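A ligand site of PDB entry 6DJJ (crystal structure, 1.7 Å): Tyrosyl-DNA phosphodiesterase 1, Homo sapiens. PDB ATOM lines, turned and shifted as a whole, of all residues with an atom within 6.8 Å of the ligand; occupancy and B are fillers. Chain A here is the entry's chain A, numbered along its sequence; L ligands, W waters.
The side-chain hydroxyl (OH) of Tyr 57 lies within hydrogen-bond range of a nitrogen (N1) of the ligand (3.3 Å).
O4 of the ligand is in hydrogen-bond range of ND2 of Asn 136, at 2.7 Å.
OG of Ser 252 is in hydrogen-bond range of O2 of the ligand, at 2.7 Å.
The side-chain amino group (NZ) of Lys 348 lies within salt-bridge range of an oxygen (O1) of the ligand (3.0 Å).
An oxygen (O3) of the ligand lies within salt-bridge range of the side-chain amino group of Lys 118, at 2.6 Å.
A ring nitrogen (NE2) of His 346 lies within hydrogen-bond range of an oxygen (O4) of the ligand (2.7 Å).
An oxygen (O1) of the ligand is in hydrogen-bond range of the side-chain amide nitrogen (ND2) of Asn 369, 3.2 Å away.
The side-chain carboxylate (OD2) of Asp 141 lies within hydrogen-bond range of the backbone NH (N) of Asn 136 (2.9 Å).
NZ of Lys 118 sits close to OD1 of Asn 56.
OD1 of Asn 136 sits at hydrogen-bond distance from N of Cys 58, at 3.0 Å.
The side-chain amino group (NZ) of Lys 118 sits at hydrogen-bond distance from the side-chain amide oxygen (OD1) of Asn 136 (3.5 Å).
NE2 of His 346 lies close to ND2 of Asn 136, at 3.5 Å.
The side-chain amide oxygen (OD1) of Asn 369 is in hydrogen-bond range of the backbone NH (N) of Ser 252 (2.9 Å).
NZ of Lys 348 sits close to ND1 of His 346 (3.4 Å).
NZ of Lys 118 lies within hydrogen-bond range of O of His 116 (2.8 Å).
Merely in contact with the ligand: His 116, Pro 314 and Ser 253.
Of the 24 residues printed, 10 come within 4 Å of the ligand.
The nearest printed residue that does not touch the ligand is Ser 312 (4.1 Å).
Water W2 lies within hydrogen-bond range of an oxygen (O2) of the ligand and the backbone carbonyl oxygen (O) of Ser 312.
Water W3 lies within hydrogen-bond range of the side-chain hydroxyl of Tyr 57 and a nitrogen (N1) of the ligand.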
ATOM      1  N   ASN A  56      32.444   5.889  -1.270  1.00  0.00           N
ATOM      2  CA  ASN A  56      32.021   4.491  -1.309  1.00  0.00           C
ATOM      3  C   ASN A  56      31.901   3.915   0.094  1.00  0.00           C
ATOM      4  O   ASN A  56      32.087   4.617   1.103  1.00  0.00           O
ATOM      5  CB  ASN A  56      32.954   3.649  -2.183  1.00  0.00           C
ATOM      6  CG  ASN A  56      32.166   2.643  -3.006  1.00  0.00           C
ATOM      7  OD1 ASN A  56      31.547   1.754  -2.440  1.00  0.00           O
ATOM      8  ND2 ASN A  56      32.108   2.845  -4.322  1.00  0.00           N
ATOM      9  N   TYR A  57      31.618   2.614   0.139  1.00  0.00           N
ATOM     10  CA  TYR A  57      31.549   1.871   1.381  1.00  0.00           C
ATOM     11  C   TYR A  57      32.797   1.031   1.601  1.00  0.00           C
ATOM     12  O   TYR A  57      33.484   1.166   2.625  1.00  0.00           O
ATOM     13  CB  TYR A  57      30.295   0.971   1.355  1.00  0.00           C
ATOM     14  CG  TYR A  57      30.294   0.022   2.529  1.00  0.00           C
ATOM     15  CD1 TYR A  57      30.019   0.490   3.801  1.00  0.00           C
ATOM     16  CD2 TYR A  57      30.614  -1.319   2.372  1.00  0.00           C
ATOM     17  CE1 TYR A  57      30.033  -0.359   4.893  1.00  0.00           C
ATOM     18  CE2 TYR A  57      30.635  -2.166   3.433  1.00  0.00           C
ATOM     19  CZ  TYR A  57      30.336  -1.692   4.693  1.00  0.00           C
ATOM     20  OH  TYR A  57      30.352  -2.555   5.758  1.00  0.00           O
ATOM     21  N   CYS A  58      33.102   0.143   0.652  1.00  0.00           N
ATOM     22  CA  CYS A  58      34.240  -0.780   0.715  1.00  0.00           C
ATOM     23  C   CYS A  58      35.245  -0.440  -0.371  1.00  0.00           C
ATOM     24  O   CYS A  58      34.872  -0.183  -1.518  1.00  0.00           O
ATOM     25  CB  CYS A  58      33.772  -2.234   0.562  1.00  0.00           C
ATOM     26  SG  CYS A  58      35.090  -3.416   0.902  1.00  0.00           S
ATOM     27  N   THR A 114      25.553   3.856   8.028  1.00  0.00           N
ATOM     28  CA  THR A 114      26.585   3.422   7.114  1.00  0.00           C
ATOM     29  C   THR A 114      26.800   4.527   6.084  1.00  0.00           C
ATOM     30  O   THR A 114      25.862   5.223   5.714  1.00  0.00           O
ATOM     31  CB  THR A 114      26.173   2.118   6.420  1.00  0.00           C
ATOM     32  OG1 THR A 114      26.000   1.101   7.405  1.00  0.00           O
ATOM     33  CG2 THR A 114      27.196   1.667   5.402  1.00  0.00           C
ATOM     34  N   HIS A 115      28.029   4.662   5.601  1.00  0.00           N
ATOM     35  CA  HIS A 115      28.273   5.512   4.431  1.00  0.00           C
ATOM     36  C   HIS A 115      28.161   4.639   3.178  1.00  0.00           C
ATOM     37  O   HIS A 115      29.133   4.022   2.747  1.00  0.00           O
ATOM     38  CB  HIS A 115      29.625   6.192   4.496  1.00  0.00           C
ATOM     39  CG  HIS A 115      29.847   7.142   3.366  1.00  0.00           C
ATOM     40  ND1 HIS A 115      30.507   6.787   2.216  1.00  0.00           N
ATOM     41  CD2 HIS A 115      29.438   8.431   3.196  1.00  0.00           C
ATOM     42  CE1 HIS A 115      30.519   7.819   1.381  1.00  0.00           C
ATOM     43  NE2 HIS A 115      29.891   8.832   1.968  1.00  0.00           N
ATOM     44  N   HIS A 116      26.958   4.574   2.616  1.00  0.00           N
ATOM     45  CA  HIS A 116      26.711   3.693   1.484  1.00  0.00           C
ATOM     46  C   HIS A 116      26.981   4.358   0.145  1.00  0.00           C
ATOM     47  O   HIS A 116      27.366   3.660  -0.810  1.00  0.00           O
ATOM     48  CB  HIS A 116      25.262   3.188   1.498  1.00  0.00           C
ATOM     49  CG  HIS A 116      25.026   2.005   2.387  1.00  0.00           C
ATOM     50  ND1 HIS A 116      24.137   2.039   3.444  1.00  0.00           N
ATOM     51  CD2 HIS A 116      25.535   0.752   2.375  1.00  0.00           C
ATOM     52  CE1 HIS A 116      24.122   0.867   4.047  1.00  0.00           C
ATOM     53  NE2 HIS A 116      24.971   0.068   3.423  1.00  0.00           N
ATOM     54  N   THR A 117      26.786   5.684   0.048  1.00  0.00           N
ATOM     55  CA  THR A 117      26.869   6.410  -1.213  1.00  0.00           C
ATOM     56  C   THR A 117      28.040   5.969  -2.086  1.00  0.00           C
ATOM     57  O   THR A 117      29.180   5.868  -1.619  1.00  0.00           O
ATOM     58  CB  THR A 117      27.017   7.904  -0.888  1.00  0.00           C
ATOM     59  OG1 THR A 117      25.784   8.363  -0.332  1.00  0.00           O
ATOM     60  CG2 THR A 117      27.363   8.715  -2.166  1.00  0.00           C
ATOM     61  N   LYS A 118      27.759   5.735  -3.369  1.00  0.00           N
ATOM     62  CA  LYS A 118      28.777   5.395  -4.358  1.00  0.00           C
ATOM     63  C   LYS A 118      28.757   6.460  -5.451  1.00  0.00           C
ATOM     64  O   LYS A 118      27.813   6.552  -6.248  1.00  0.00           O
ATOM     65  CB  LYS A 118      28.543   3.998  -4.918  1.00  0.00           C
ATOM     66  CG  LYS A 118      28.777   2.922  -3.837  1.00  0.00           C
ATOM     67  CD  LYS A 118      27.527   2.100  -3.624  1.00  0.00           C
ATOM     68  CE  LYS A 118      27.806   0.826  -2.836  1.00  0.00           C
ATOM     69  NZ  LYS A 118      28.312   1.080  -1.477  1.00  0.00           N
ATOM     70  N   THR A 134      26.470   2.093  -8.253  1.00  0.00           N
ATOM     71  CA  THR A 134      26.097   1.191  -7.171  1.00  0.00           C
ATOM     72  C   THR A 134      27.196   0.235  -6.725  1.00  0.00           C
ATOM     73  O   THR A 134      26.932  -0.601  -5.846  1.00  0.00           O
ATOM     74  CB  THR A 134      24.856   0.357  -7.561  1.00  0.00           C
ATOM     75  OG1 THR A 134      25.180  -0.534  -8.642  1.00  0.00           O
ATOM     76  CG2 THR A 134      23.706   1.266  -7.990  1.00  0.00           C
ATOM     77  N   SER A 135      28.402   0.338  -7.241  1.00  0.00           N
ATOM     78  CA  SER A 135      29.436  -0.676  -7.015  1.00  0.00           C
ATOM     79  C   SER A 135      30.436  -0.232  -5.973  1.00  0.00           C
ATOM     80  O   SER A 135      30.919   0.903  -6.011  1.00  0.00           O
ATOM     81  CB  SER A 135      30.196  -1.010  -8.292  1.00  0.00           C
ATOM     82  OG  SER A 135      29.340  -1.496  -9.301  1.00  0.00           O
ATOM     83  N   ASN A 136      30.786  -1.148  -5.064  1.00  0.00           N
ATOM     84  CA  ASN A 136      31.942  -0.960  -4.208  1.00  0.00           C
ATOM     85  C   ASN A 136      33.219  -0.978  -5.052  1.00  0.00           C
ATOM     86  O   ASN A 136      33.232  -1.443  -6.187  1.00  0.00           O
ATOM     87  CB  ASN A 136      31.999  -2.064  -3.142  1.00  0.00           C
ATOM     88  CG  ASN A 136      30.889  -1.905  -2.102  1.00  0.00           C
ATOM     89  OD1 ASN A 136      31.004  -1.104  -1.177  1.00  0.00           O
ATOM     90  ND2 ASN A 136      29.802  -2.666  -2.266  1.00  0.00           N
ATOM     91  N   ASP A 141      32.832  -6.573  -7.195  1.00  0.00           N
ATOM     92  CA  ASP A 141      31.617  -5.818  -7.504  1.00  0.00           C
ATOM     93  C   ASP A 141      31.515  -5.430  -8.969  1.00  0.00           C
ATOM     94  O   ASP A 141      30.417  -5.103  -9.430  1.00  0.00           O
ATOM     95  CB  ASP A 141      31.529  -4.561  -6.610  1.00  0.00           C
ATOM     96  CG  ASP A 141      30.698  -4.798  -5.372  1.00  0.00           C
ATOM     97  OD1 ASP A 141      30.801  -5.914  -4.804  1.00  0.00           O
ATOM     98  OD2 ASP A 141      29.938  -3.876  -4.982  1.00  0.00           O
ATOM     99  N   PHE A 251      16.520  -4.564  -4.834  1.00  0.00           N
ATOM    100  CA  PHE A 251      17.556  -4.200  -3.853  1.00  0.00           C
ATOM    101  C   PHE A 251      18.394  -5.417  -3.536  1.00  0.00           C
ATOM    102  O   PHE A 251      18.049  -6.552  -3.918  1.00  0.00           O
ATOM    103  CB  PHE A 251      16.907  -3.652  -2.570  1.00  0.00           C
ATOM    104  CG  PHE A 251      15.705  -4.442  -2.166  1.00  0.00           C
ATOM    105  CD1 PHE A 251      15.854  -5.621  -1.460  1.00  0.00           C
ATOM    106  CD2 PHE A 251      14.426  -4.064  -2.584  1.00  0.00           C
ATOM    107  CE1 PHE A 251      14.748  -6.387  -1.125  1.00  0.00           C
ATOM    108  CE2 PHE A 251      13.320  -4.820  -2.258  1.00  0.00           C
ATOM    109  CZ  PHE A 251      13.489  -5.994  -1.527  1.00  0.00           C
ATOM    110  N   SER A 252      19.492  -5.187  -2.820  1.00  0.00           N
ATOM    111  CA  SER A 252      20.425  -6.258  -2.466  1.00  0.00           C
ATOM    112  C   SER A 252      20.488  -6.522  -0.963  1.00  0.00           C
ATOM    113  O   SER A 252      21.182  -7.448  -0.550  1.00  0.00           O
ATOM    114  CB  SER A 252      21.826  -5.945  -3.001  1.00  0.00           C
ATOM    115  OG  SER A 252      22.360  -4.753  -2.424  1.00  0.00           O
ATOM    116  N   SER A 253      19.761  -5.762  -0.151  1.00  0.00           N
ATOM    117  CA  SER A 253      19.771  -5.972   1.290  1.00  0.00           C
ATOM    118  C   SER A 253      18.439  -5.508   1.851  1.00  0.00           C
ATOM    119  O   SER A 253      17.730  -4.689   1.244  1.00  0.00           O
ATOM    120  CB  SER A 253      20.949  -5.250   1.945  1.00  0.00           C
ATOM    121  OG  SER A 253      21.125  -5.701   3.268  1.00  0.00           O
ATOM    122  N   SER A 312      27.360 -10.709  -0.875  1.00  0.00           N
ATOM    123  CA  SER A 312      26.979  -9.345  -1.210  1.00  0.00           C
ATOM    124  C   SER A 312      25.471  -9.153  -1.195  1.00  0.00           C
ATOM    125  O   SER A 312      24.958  -8.177  -1.752  1.00  0.00           O
ATOM    126  CB  SER A 312      27.565  -8.963  -2.569  1.00  0.00           C
ATOM    127  OG  SER A 312      28.981  -8.913  -2.483  1.00  0.00           O
ATOM    128  N   LEU A 313      24.738 -10.078  -0.563  1.00  0.00           N
ATOM    129  CA  LEU A 313      23.297  -9.979  -0.370  1.00  0.00           C
ATOM    130  C   LEU A 313      23.034 -10.179   1.119  1.00  0.00           C
ATOM    131  O   LEU A 313      22.586 -11.245   1.553  1.00  0.00           O
ATOM    132  CB  LEU A 313      22.547 -11.010  -1.214  1.00  0.00           C
ATOM    133  CG  LEU A 313      22.671 -10.826  -2.740  1.00  0.00           C
ATOM    134  CD1 LEU A 313      22.426 -12.143  -3.497  1.00  0.00           C
ATOM    135  CD2 LEU A 313      21.690  -9.756  -3.240  1.00  0.00           C
ATOM    136  N   PRO A 314      23.351  -9.173   1.946  1.00  0.00           N
ATOM    137  CA  PRO A 314      23.509  -9.423   3.411  1.00  0.00           C
ATOM    138  C   PRO A 314      22.232  -9.319   4.244  1.00  0.00           C
ATOM    139  O   PRO A 314      22.113  -8.500   5.160  1.00  0.00           O
ATOM    140  CB  PRO A 314      24.546  -8.376   3.806  1.00  0.00           C
ATOM    141  CG  PRO A 314      24.374  -7.267   2.841  1.00  0.00           C
ATOM    142  CD  PRO A 314      23.867  -7.859   1.539  1.00  0.00           C
ATOM    143  N   PRO A 345      22.181  -9.171  -8.583  1.00  0.00           N
ATOM    144  CA  PRO A 345      22.063  -7.710  -8.514  1.00  0.00           C
ATOM    145  C   PRO A 345      22.714  -7.133  -7.264  1.00  0.00           C
ATOM    146  O   PRO A 345      22.445  -7.563  -6.141  1.00  0.00           O
ATOM    147  CB  PRO A 345      20.551  -7.484  -8.492  1.00  0.00           C
ATOM    148  CG  PRO A 345      19.985  -8.744  -7.849  1.00  0.00           C
ATOM    149  CD  PRO A 345      20.886  -9.853  -8.379  1.00  0.00           C
ATOM    150  N   HIS A 346      23.568  -6.123  -7.471  1.00  0.00           N
ATOM    151  CA  HIS A 346      23.941  -5.211  -6.414  1.00  0.00           C
ATOM    152  C   HIS A 346      23.470  -3.796  -6.725  1.00  0.00           C
ATOM    153  O   HIS A 346      23.576  -2.900  -5.884  1.00  0.00           O
ATOM    154  CB  HIS A 346      25.465  -5.276  -6.180  1.00  0.00           C
ATOM    155  CG  HIS A 346      25.945  -4.495  -4.993  1.00  0.00           C
ATOM    156  ND1 HIS A 346      26.423  -3.211  -5.098  1.00  0.00           N
ATOM    157  CD2 HIS A 346      26.040  -4.832  -3.683  1.00  0.00           C
ATOM    158  CE1 HIS A 346      26.778  -2.775  -3.903  1.00  0.00           C
ATOM    159  NE2 HIS A 346      26.564  -3.748  -3.024  1.00  0.00           N
ATOM    160  N   LYS A 348      20.447  -1.100  -7.066  1.00  0.00           N
ATOM    161  CA  LYS A 348      19.149  -0.911  -6.423  1.00  0.00           C
ATOM    162  C   LYS A 348      18.347   0.007  -7.316  1.00  0.00           C
ATOM    163  O   LYS A 348      18.865   1.020  -7.784  1.00  0.00           O
ATOM    164  CB  LYS A 348      19.259  -0.282  -5.039  1.00  0.00           C
ATOM    165  CG  LYS A 348      20.008  -1.084  -3.989  1.00  0.00           C
ATOM    166  CD  LYS A 348      21.511  -0.874  -4.115  1.00  0.00           C
ATOM    167  CE  LYS A 348      22.219  -1.775  -3.141  1.00  0.00           C
ATOM    168  NZ  LYS A 348      23.530  -2.174  -3.647  1.00  0.00           N
ATOM    169  N   SER A 367      21.846   3.945  -4.243  1.00  0.00           N
ATOM    170  CA  SER A 367      22.486   3.042  -3.296  1.00  0.00           C
ATOM    171  C   SER A 367      21.510   2.495  -2.266  1.00  0.00           C
ATOM    172  O   SER A 367      21.846   1.520  -1.584  1.00  0.00           O
ATOM    173  CB  SER A 367      23.611   3.786  -2.559  1.00  0.00           C
ATOM    174  OG  SER A 367      23.098   4.915  -1.873  1.00  0.00           O
ATOM    175  N   ASN A 369      19.028   0.545  -0.126  1.00  0.00           N
ATOM    176  CA  ASN A 369      18.352  -0.742  -0.016  1.00  0.00           C
ATOM    177  C   ASN A 369      16.993  -0.591   0.665  1.00  0.00           C
ATOM    178  O   ASN A 369      16.547   0.517   0.967  1.00  0.00           O
ATOM    179  CB  ASN A 369      19.242  -1.723   0.754  1.00  0.00           C
ATOM    180  CG  ASN A 369      20.280  -2.319  -0.119  1.00  0.00           C
ATOM    181  OD1 ASN A 369      19.971  -2.798  -1.217  1.00  0.00           O
ATOM    182  ND2 ASN A 369      21.538  -2.313   0.339  1.00  0.00           N
ATOM    183  N   TRP A 443      21.988 -14.765   4.243  1.00  0.00           N
ATOM    184  CA  TRP A 443      23.398 -15.004   3.982  1.00  0.00           C
ATOM    185  C   TRP A 443      24.115 -15.749   5.090  1.00  0.00           C
ATOM    186  O   TRP A 443      25.224 -16.248   4.842  1.00  0.00           O
ATOM    187  CB  TRP A 443      24.151 -13.694   3.697  1.00  0.00           C
ATOM    188  CG  TRP A 443      24.421 -12.781   4.862  1.00  0.00           C
ATOM    189  CD1 TRP A 443      23.723 -12.685   6.035  1.00  0.00           C
ATOM    190  CD2 TRP A 443      25.467 -11.801   4.934  1.00  0.00           C
ATOM    191  NE1 TRP A 443      24.275 -11.711   6.844  1.00  0.00           N
ATOM    192  CE2 TRP A 443      25.347 -11.152   6.192  1.00  0.00           C
ATOM    193  CE3 TRP A 443      26.496 -11.407   4.068  1.00  0.00           C
ATOM    194  CZ2 TRP A 443      26.226 -10.141   6.594  1.00  0.00           C
ATOM    195  CZ3 TRP A 443      27.371 -10.399   4.478  1.00  0.00           C
ATOM    196  CH2 TRP A 443      27.225  -9.782   5.724  1.00  0.00           C
HETATM  197  C1  LIG L   1      27.232  -1.935   0.218  1.00  0.00           C
HETATM  198  C2  LIG L   1      27.111  -2.444   2.648  1.00  0.00           C
HETATM  199  C3  LIG L   1      26.506  -3.001   3.769  1.00  0.00           C
HETATM  200  C4  LIG L   1      25.293  -3.649   3.650  1.00  0.00           C
HETATM  201  C5  LIG L   1      24.696  -3.757   2.412  1.00  0.00           C
HETATM  202  C6  LIG L   1      25.311  -3.230   1.288  1.00  0.00           C
HETATM  203  C7  LIG L   1      24.588  -3.354  -0.061  1.00  0.00           C
HETATM  204  C8  LIG L   1      26.507  -2.544   1.409  1.00  0.00           C
HETATM  205  N1  LIG L   1      27.147  -2.879   5.072  1.00  0.00           N
HETATM  206  O1  LIG L   1      24.489  -2.353  -0.802  1.00  0.00           O
HETATM  207  O2  LIG L   1      24.065  -4.449  -0.391  1.00  0.00           O
HETATM  208  O3  LIG L   1      27.588  -0.731   0.270  1.00  0.00           O
HETATM  209  O4  LIG L   1      27.500  -2.623  -0.789  1.00  0.00           O
HETATM  210  O   HOH W   1      26.912  -5.885   6.361  1.00  0.00           O
HETATM  211  O   HOH W   2      26.679  -6.073  -0.306  1.00  0.00           O
HETATM  212  O   HOH W   3      28.751  -1.885   7.958  1.00  0.00           O
